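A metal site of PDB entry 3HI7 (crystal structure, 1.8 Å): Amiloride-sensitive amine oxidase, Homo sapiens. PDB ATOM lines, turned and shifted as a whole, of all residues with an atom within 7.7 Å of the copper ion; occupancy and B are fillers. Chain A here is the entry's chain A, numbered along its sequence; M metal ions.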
ATOM      1  N   ALA A 337     -22.926 -30.698   1.631  1.00  0.00           N
ATOM      2  CA  ALA A 337     -23.594 -30.521   0.366  1.00  0.00           C
ATOM      3  C   ALA A 337     -24.816 -31.441   0.384  1.00  0.00           C
ATOM      4  O   ALA A 337     -24.676 -32.655   0.522  1.00  0.00           O
ATOM      5  CB  ALA A 337     -22.637 -30.834  -0.819  1.00  0.00           C
ATOM      6  N   TYR A 339     -28.209 -32.784  -1.340  1.00  0.00           N
ATOM      7  CA  TYR A 339     -28.677 -33.019  -2.698  1.00  0.00           C
ATOM      8  C   TYR A 339     -30.136 -33.479  -2.787  1.00  0.00           C
ATOM      9  O   TYR A 339     -30.704 -34.031  -1.846  1.00  0.00           O
ATOM     10  CB  TYR A 339     -27.784 -34.096  -3.371  1.00  0.00           C
ATOM     11  CG  TYR A 339     -26.381 -33.629  -3.648  1.00  0.00           C
ATOM     12  CD1 TYR A 339     -26.025 -33.117  -4.898  1.00  0.00           C
ATOM     13  CD2 TYR A 339     -25.408 -33.668  -2.663  1.00  0.00           C
ATOM     14  CE1 TYR A 339     -24.748 -32.638  -5.155  1.00  0.00           C
ATOM     15  CE2 TYR A 339     -24.113 -33.181  -2.905  1.00  0.00           C
ATOM     16  CZ  TYR A 339     -23.792 -32.665  -4.135  1.00  0.00           C
ATOM     17  OH  TYR A 339     -22.506 -32.203  -4.355  1.00  0.00           O
ATOM     18  N   ASN A 440     -14.339 -35.321  -5.334  1.00  0.00           N
ATOM     19  CA  ASN A 440     -14.653 -34.585  -6.568  1.00  0.00           C
ATOM     20  C   ASN A 440     -14.390 -33.086  -6.464  1.00  0.00           C
ATOM     21  O   ASN A 440     -13.870 -32.463  -7.414  1.00  0.00           O
ATOM     22  CB  ASN A 440     -16.103 -34.832  -7.021  1.00  0.00           C
ATOM     23  CG  ASN A 440     -17.124 -34.587  -5.917  1.00  0.00           C
ATOM     24  OD1 ASN A 440     -17.041 -35.208  -4.853  1.00  0.00           O
ATOM     25  ND2 ASN A 440     -18.106 -33.701  -6.174  1.00  0.00           N
ATOM     26  N   TPQ A 441     -14.767 -32.497  -5.320  1.00  0.00           N
ATOM     27  CA  TPQ A 441     -14.717 -31.052  -5.141  1.00  0.00           C
ATOM     28  CB  TPQ A 441     -15.832 -30.549  -4.183  1.00  0.00           C
ATOM     29  C   TPQ A 441     -13.405 -30.622  -4.506  1.00  0.00           C
ATOM     30  O   TPQ A 441     -12.847 -31.333  -3.664  1.00  0.00           O
ATOM     31  C1  TPQ A 441     -17.111 -30.094  -4.851  1.00  0.00           C
ATOM     32  C2  TPQ A 441     -18.396 -30.640  -4.352  1.00  0.00           C
ATOM     33  O2  TPQ A 441     -18.412 -31.466  -3.409  1.00  0.00           O
ATOM     34  C3  TPQ A 441     -19.662 -30.185  -4.970  1.00  0.00           C
ATOM     35  C4  TPQ A 441     -19.659 -29.261  -6.002  1.00  0.00           C
ATOM     36  O4  TPQ A 441     -20.725 -28.885  -6.531  1.00  0.00           O
ATOM     37  C5  TPQ A 441     -18.387 -28.724  -6.508  1.00  0.00           C
ATOM     38  O5  TPQ A 441     -18.411 -27.901  -7.442  1.00  0.00           O
ATOM     39  C6  TPQ A 441     -17.121 -29.179  -5.890  1.00  0.00           C
ATOM     40  N   TYR A 443     -12.236 -27.422  -2.309  1.00  0.00           N
ATOM     41  CA  TYR A 443     -12.519 -26.161  -1.619  1.00  0.00           C
ATOM     42  C   TYR A 443     -11.237 -25.486  -1.255  1.00  0.00           C
ATOM     43  O   TYR A 443     -10.280 -26.127  -0.796  1.00  0.00           O
ATOM     44  CB  TYR A 443     -13.326 -26.390  -0.342  1.00  0.00           C
ATOM     45  CG  TYR A 443     -14.721 -26.944  -0.559  1.00  0.00           C
ATOM     46  CD1 TYR A 443     -15.323 -26.971  -1.813  1.00  0.00           C
ATOM     47  CD2 TYR A 443     -15.446 -27.398   0.523  1.00  0.00           C
ATOM     48  CE1 TYR A 443     -16.622 -27.500  -1.984  1.00  0.00           C
ATOM     49  CE2 TYR A 443     -16.718 -27.908   0.365  1.00  0.00           C
ATOM     50  CZ  TYR A 443     -17.297 -27.972  -0.896  1.00  0.00           C
ATOM     51  OH  TYR A 443     -18.560 -28.496  -1.039  1.00  0.00           O
ATOM     52  N   ALA A 461     -15.311 -22.606  -3.978  1.00  0.00           N
ATOM     53  CA  ALA A 461     -15.540 -23.965  -4.483  1.00  0.00           C
ATOM     54  C   ALA A 461     -15.111 -24.126  -5.931  1.00  0.00           C
ATOM     55  O   ALA A 461     -15.428 -23.292  -6.772  1.00  0.00           O
ATOM     56  CB  ALA A 461     -17.026 -24.350  -4.330  1.00  0.00           C
ATOM     57  N   THR A 462     -14.360 -25.195  -6.201  1.00  0.00           N
ATOM     58  CA  THR A 462     -13.998 -25.591  -7.554  1.00  0.00           C
ATOM     59  C   THR A 462     -13.898 -27.125  -7.609  1.00  0.00           C
ATOM     60  O   THR A 462     -14.389 -27.795  -6.728  1.00  0.00           O
ATOM     61  CB  THR A 462     -12.740 -24.813  -8.045  1.00  0.00           C
ATOM     62  OG1 THR A 462     -12.480 -25.126  -9.422  1.00  0.00           O
ATOM     63  CG2 THR A 462     -11.506 -25.067  -7.160  1.00  0.00           C
ATOM     64  N   TYR A 464     -14.935 -30.901  -9.439  1.00  0.00           N
ATOM     65  CA  TYR A 464     -16.001 -31.536 -10.223  1.00  0.00           C
ATOM     66  C   TYR A 464     -17.279 -31.635  -9.400  1.00  0.00           C
ATOM     67  O   TYR A 464     -17.197 -31.902  -8.217  1.00  0.00           O
ATOM     68  CB  TYR A 464     -15.593 -32.982 -10.567  1.00  0.00           C
ATOM     69  CG  TYR A 464     -14.518 -33.121 -11.623  1.00  0.00           C
ATOM     70  CD1 TYR A 464     -13.190 -33.166 -11.271  1.00  0.00           C
ATOM     71  CD2 TYR A 464     -14.865 -33.250 -12.978  1.00  0.00           C
ATOM     72  CE1 TYR A 464     -12.197 -33.295 -12.239  1.00  0.00           C
ATOM     73  CE2 TYR A 464     -13.881 -33.390 -13.943  1.00  0.00           C
ATOM     74  CZ  TYR A 464     -12.549 -33.421 -13.557  1.00  0.00           C
ATOM     75  OH  TYR A 464     -11.546 -33.567 -14.487  1.00  0.00           O
ATOM     76  N   VAL A 465     -18.428 -31.437 -10.031  1.00  0.00           N
ATOM     77  CA  VAL A 465     -19.728 -31.608  -9.368  1.00  0.00           C
ATOM     78  C   VAL A 465     -20.080 -33.084  -9.139  1.00  0.00           C
ATOM     79  O   VAL A 465     -19.525 -33.975  -9.790  1.00  0.00           O
ATOM     80  CB  VAL A 465     -20.893 -30.971 -10.165  1.00  0.00           C
ATOM     81  CG1 VAL A 465     -20.619 -29.474 -10.363  1.00  0.00           C
ATOM     82  CG2 VAL A 465     -21.123 -31.688 -11.511  1.00  0.00           C
ATOM     83  N   HIS A 466     -20.991 -33.324  -8.198  1.00  0.00           N
ATOM     84  CA  HIS A 466     -21.564 -34.644  -7.921  1.00  0.00           C
ATOM     85  C   HIS A 466     -22.705 -34.804  -8.913  1.00  0.00           C
ATOM     86  O   HIS A 466     -23.615 -33.946  -9.007  1.00  0.00           O
ATOM     87  CB  HIS A 466     -22.049 -34.659  -6.475  1.00  0.00           C
ATOM     88  CG  HIS A 466     -22.692 -35.943  -6.032  1.00  0.00           C
ATOM     89  ND1 HIS A 466     -22.049 -37.165  -6.059  1.00  0.00           N
ATOM     90  CD2 HIS A 466     -23.884 -36.153  -5.408  1.00  0.00           C
ATOM     91  CE1 HIS A 466     -22.832 -38.075  -5.525  1.00  0.00           C
ATOM     92  NE2 HIS A 466     -23.950 -37.488  -5.106  1.00  0.00           N
ATOM     93  N   ASN A 488     -26.906 -32.718 -10.246  1.00  0.00           N
ATOM     94  CA  ASN A 488     -27.933 -32.656  -9.205  1.00  0.00           C
ATOM     95  C   ASN A 488     -27.933 -31.321  -8.463  1.00  0.00           C
ATOM     96  O   ASN A 488     -26.856 -30.783  -8.122  1.00  0.00           O
ATOM     97  CB  ASN A 488     -27.750 -33.778  -8.165  1.00  0.00           C
ATOM     98  CG  ASN A 488     -27.955 -35.168  -8.767  1.00  0.00           C
ATOM     99  OD1 ASN A 488     -27.212 -35.567  -9.655  1.00  0.00           O
ATOM    100  ND2 ASN A 488     -28.901 -35.923  -8.225  1.00  0.00           N
ATOM    101  N   ILE A 489     -29.132 -30.803  -8.231  1.00  0.00           N
ATOM    102  CA  ILE A 489     -29.328 -29.620  -7.383  1.00  0.00           C
ATOM    103  C   ILE A 489     -28.862 -29.925  -5.970  1.00  0.00           C
ATOM    104  O   ILE A 489     -29.032 -31.047  -5.477  1.00  0.00           O
ATOM    105  CB  ILE A 489     -30.830 -29.219  -7.346  1.00  0.00           C
ATOM    106  CG1 ILE A 489     -31.010 -27.827  -6.730  1.00  0.00           C
ATOM    107  CG2 ILE A 489     -31.667 -30.290  -6.620  1.00  0.00           C
ATOM    108  CD1 ILE A 489     -32.459 -27.244  -6.882  1.00  0.00           C
ATOM    109  N   HIS A 490     -28.216 -28.952  -5.335  1.00  0.00           N
ATOM    110  CA  HIS A 490     -27.796 -29.091  -3.950  1.00  0.00           C
ATOM    111  C   HIS A 490     -27.541 -27.720  -3.342  1.00  0.00           C
ATOM    112  O   HIS A 490     -27.431 -26.734  -4.044  1.00  0.00           O
ATOM    113  CB  HIS A 490     -26.521 -29.905  -3.852  1.00  0.00           C
ATOM    114  CG  HIS A 490     -25.425 -29.370  -4.700  1.00  0.00           C
ATOM    115  ND1 HIS A 490     -25.466 -29.421  -6.072  1.00  0.00           N
ATOM    116  CD2 HIS A 490     -24.271 -28.732  -4.380  1.00  0.00           C
ATOM    117  CE1 HIS A 490     -24.379 -28.855  -6.559  1.00  0.00           C
ATOM    118  NE2 HIS A 490     -23.638 -28.418  -5.554  1.00  0.00           N
ATOM    119  N   THR A 491     -27.368 -27.712  -2.033  1.00  0.00           N
ATOM    120  CA  THR A 491     -26.960 -26.509  -1.317  1.00  0.00           C
ATOM    121  C   THR A 491     -25.688 -26.796  -0.571  1.00  0.00           C
ATOM    122  O   THR A 491     -25.591 -27.811   0.112  1.00  0.00           O
ATOM    123  CB  THR A 491     -28.072 -26.079  -0.351  1.00  0.00           C
ATOM    124  OG1 THR A 491     -29.300 -25.886  -1.079  1.00  0.00           O
ATOM    125  CG2 THR A 491     -27.713 -24.760   0.388  1.00  0.00           C
ATOM    126  N   HIS A 492     -24.710 -25.894  -0.705  1.00  0.00           N
ATOM    127  CA  HIS A 492     -23.516 -25.919   0.092  1.00  0.00           C
ATOM    128  C   HIS A 492     -23.754 -25.136   1.369  1.00  0.00           C
ATOM    129  O   HIS A 492     -24.236 -24.012   1.308  1.00  0.00           O
ATOM    130  CB  HIS A 492     -22.355 -25.243  -0.629  1.00  0.00           C
ATOM    131  CG  HIS A 492     -21.861 -25.980  -1.824  1.00  0.00           C
ATOM    132  ND1 HIS A 492     -20.823 -26.884  -1.780  1.00  0.00           N
ATOM    133  CD2 HIS A 492     -22.251 -25.927  -3.125  1.00  0.00           C
ATOM    134  CE1 HIS A 492     -20.602 -27.366  -2.984  1.00  0.00           C
ATOM    135  NE2 HIS A 492     -21.442 -26.789  -3.820  1.00  0.00           N
ATOM    136  N   PHE A 653     -24.596 -21.492  -0.149  1.00  0.00           N
ATOM    137  CA  PHE A 653     -25.248 -21.152  -1.404  1.00  0.00           C
ATOM    138  C   PHE A 653     -25.931 -22.338  -2.058  1.00  0.00           C
ATOM    139  O   PHE A 653     -25.421 -23.472  -1.990  1.00  0.00           O
ATOM    140  CB  PHE A 653     -24.296 -20.464  -2.391  1.00  0.00           C
ATOM    141  CG  PHE A 653     -23.092 -21.287  -2.837  1.00  0.00           C
ATOM    142  CD1 PHE A 653     -23.101 -21.972  -4.040  1.00  0.00           C
ATOM    143  CD2 PHE A 653     -21.921 -21.294  -2.082  1.00  0.00           C
ATOM    144  CE1 PHE A 653     -21.969 -22.680  -4.464  1.00  0.00           C
ATOM    145  CE2 PHE A 653     -20.802 -22.006  -2.488  1.00  0.00           C
ATOM    146  CZ  PHE A 653     -20.828 -22.693  -3.683  1.00  0.00           C
ATOM    147  N   LEU A 654     -27.091 -22.077  -2.650  1.00  0.00           N
ATOM    148  CA  LEU A 654     -27.741 -23.007  -3.559  1.00  0.00           C
ATOM    149  C   LEU A 654     -26.922 -23.091  -4.851  1.00  0.00           C
ATOM    150  O   LEU A 654     -26.532 -22.076  -5.428  1.00  0.00           O
ATOM    151  CB  LEU A 654     -29.184 -22.543  -3.893  1.00  0.00           C
ATOM    152  CG  LEU A 654     -29.975 -23.411  -4.891  1.00  0.00           C
ATOM    153  CD1 LEU A 654     -30.311 -24.783  -4.300  1.00  0.00           C
ATOM    154  CD2 LEU A 654     -31.254 -22.667  -5.316  1.00  0.00           C
ATOM    155  N   HIS A 655     -26.669 -24.320  -5.294  1.00  0.00           N
ATOM    156  CA  HIS A 655     -25.956 -24.572  -6.527  1.00  0.00           C
ATOM    157  C   HIS A 655     -26.845 -25.453  -7.431  1.00  0.00           C
ATOM    158  O   HIS A 655     -27.001 -26.664  -7.210  1.00  0.00           O
ATOM    159  CB  HIS A 655     -24.615 -25.263  -6.259  1.00  0.00           C
ATOM    160  CG  HIS A 655     -23.763 -25.511  -7.482  1.00  0.00           C
ATOM    161  ND1 HIS A 655     -22.590 -26.219  -7.427  1.00  0.00           N
ATOM    162  CD2 HIS A 655     -23.928 -25.163  -8.790  1.00  0.00           C
ATOM    163  CE1 HIS A 655     -22.046 -26.269  -8.631  1.00  0.00           C
ATOM    164  NE2 HIS A 655     -22.847 -25.656  -9.491  1.00  0.00           N
ATOM    165  N   ILE A 656     -27.445 -24.806  -8.422  1.00  0.00           N
ATOM    166  CA  ILE A 656     -28.134 -25.500  -9.508  1.00  0.00           C
ATOM    167  C   ILE A 656     -27.101 -25.600 -10.616  1.00  0.00           C
ATOM    168  O   ILE A 656     -26.720 -24.577 -11.188  1.00  0.00           O
ATOM    169  CB  ILE A 656     -29.356 -24.698 -10.010  1.00  0.00           C
ATOM    170  CG1 ILE A 656     -30.405 -24.548  -8.897  1.00  0.00           C
ATOM    171  CG2 ILE A 656     -29.973 -25.401 -11.248  1.00  0.00           C
ATOM    172  CD1 ILE A 656     -31.525 -23.528  -9.241  1.00  0.00           C
ATOM    173  N   PRO A 657     -26.621 -26.828 -10.913  1.00  0.00           N
ATOM    174  CA  PRO A 657     -25.538 -26.858 -11.898  1.00  0.00           C
ATOM    175  C   PRO A 657     -25.979 -26.394 -13.284  1.00  0.00           C
ATOM    176  O   PRO A 657     -27.171 -26.407 -13.624  1.00  0.00           O
ATOM    177  CB  PRO A 657     -25.118 -28.329 -11.901  1.00  0.00           C
ATOM    178  CG  PRO A 657     -25.477 -28.813 -10.532  1.00  0.00           C
ATOM    179  CD  PRO A 657     -26.755 -28.112 -10.205  1.00  0.00           C
ATOM    180  N   ASP A 661     -20.303 -25.466 -15.726  1.00  0.00           N
ATOM    181  CA  ASP A 661     -19.671 -26.268 -14.665  1.00  0.00           C
ATOM    182  C   ASP A 661     -18.890 -27.476 -15.213  1.00  0.00           C
ATOM    183  O   ASP A 661     -18.348 -28.235 -14.440  1.00  0.00           O
ATOM    184  CB  ASP A 661     -20.705 -26.809 -13.668  1.00  0.00           C
ATOM    185  CG  ASP A 661     -21.192 -25.786 -12.632  1.00  0.00           C
ATOM    186  OD1 ASP A 661     -20.419 -24.934 -12.184  1.00  0.00           O
ATOM    187  OD2 ASP A 661     -22.377 -25.899 -12.244  1.00  0.00           O
ATOM    188  N   THR A 665     -16.602 -26.724 -11.773  1.00  0.00           N
ATOM    189  CA  THR A 665     -17.088 -25.495 -11.167  1.00  0.00           C
ATOM    190  C   THR A 665     -15.905 -24.525 -11.088  1.00  0.00           C
ATOM    191  O   THR A 665     -14.749 -24.943 -10.895  1.00  0.00           O
ATOM    192  CB  THR A 665     -17.613 -25.769  -9.758  1.00  0.00           C
ATOM    193  OG1 THR A 665     -18.686 -26.696  -9.828  1.00  0.00           O
ATOM    194  CG2 THR A 665     -18.089 -24.485  -9.067  1.00  0.00           C
ATOM    195  N   ASN A 670     -18.349 -17.853  -6.675  1.00  0.00           N
ATOM    196  CA  ASN A 670     -18.651 -19.086  -5.953  1.00  0.00           C
ATOM    197  C   ASN A 670     -17.868 -19.115  -4.642  1.00  0.00           C
ATOM    198  O   ASN A 670     -17.266 -20.148  -4.286  1.00  0.00           O
ATOM    199  CB  ASN A 670     -18.309 -20.336  -6.797  1.00  0.00           C
ATOM    200  CG  ASN A 670     -19.457 -20.779  -7.698  1.00  0.00           C
ATOM    201  OD1 ASN A 670     -20.621 -20.618  -7.353  1.00  0.00           O
ATOM    202  ND2 ASN A 670     -19.124 -21.395  -8.870  1.00  0.00           N
HETATM  203 CU    CU M   1     -21.914 -27.240  -5.803  1.00  0.00          CU
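A ring nitrogen (NE2) of His 655 is in hydrogen-bond range of the side-chain carboxylate of Asp 661 (2.8 Å). OG1 of Thr 665 sits at hydrogen-bond distance from O5 of TPQ 441, at 2.7 Å. A ring nitrogen (ND1) of His 490 lies within hydrogen-bond range of the backbone carbonyl oxygen (O) of Asn 488 (2.8 Å). The backbone NH (N) of His 492 is in hydrogen-bond range of the backbone carbonyl oxygen (O) of Phe 653, at 2.8 Å. A ring nitrogen (ND1) of His 492 is in hydrogen-bond range of the side-chain hydroxyl of Tyr 443, 2.9 Å away.
The copper ion is bound by ND1 of His 655, NE2 of His 492, NE2 of His 490 and O4 of TPQ 441.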
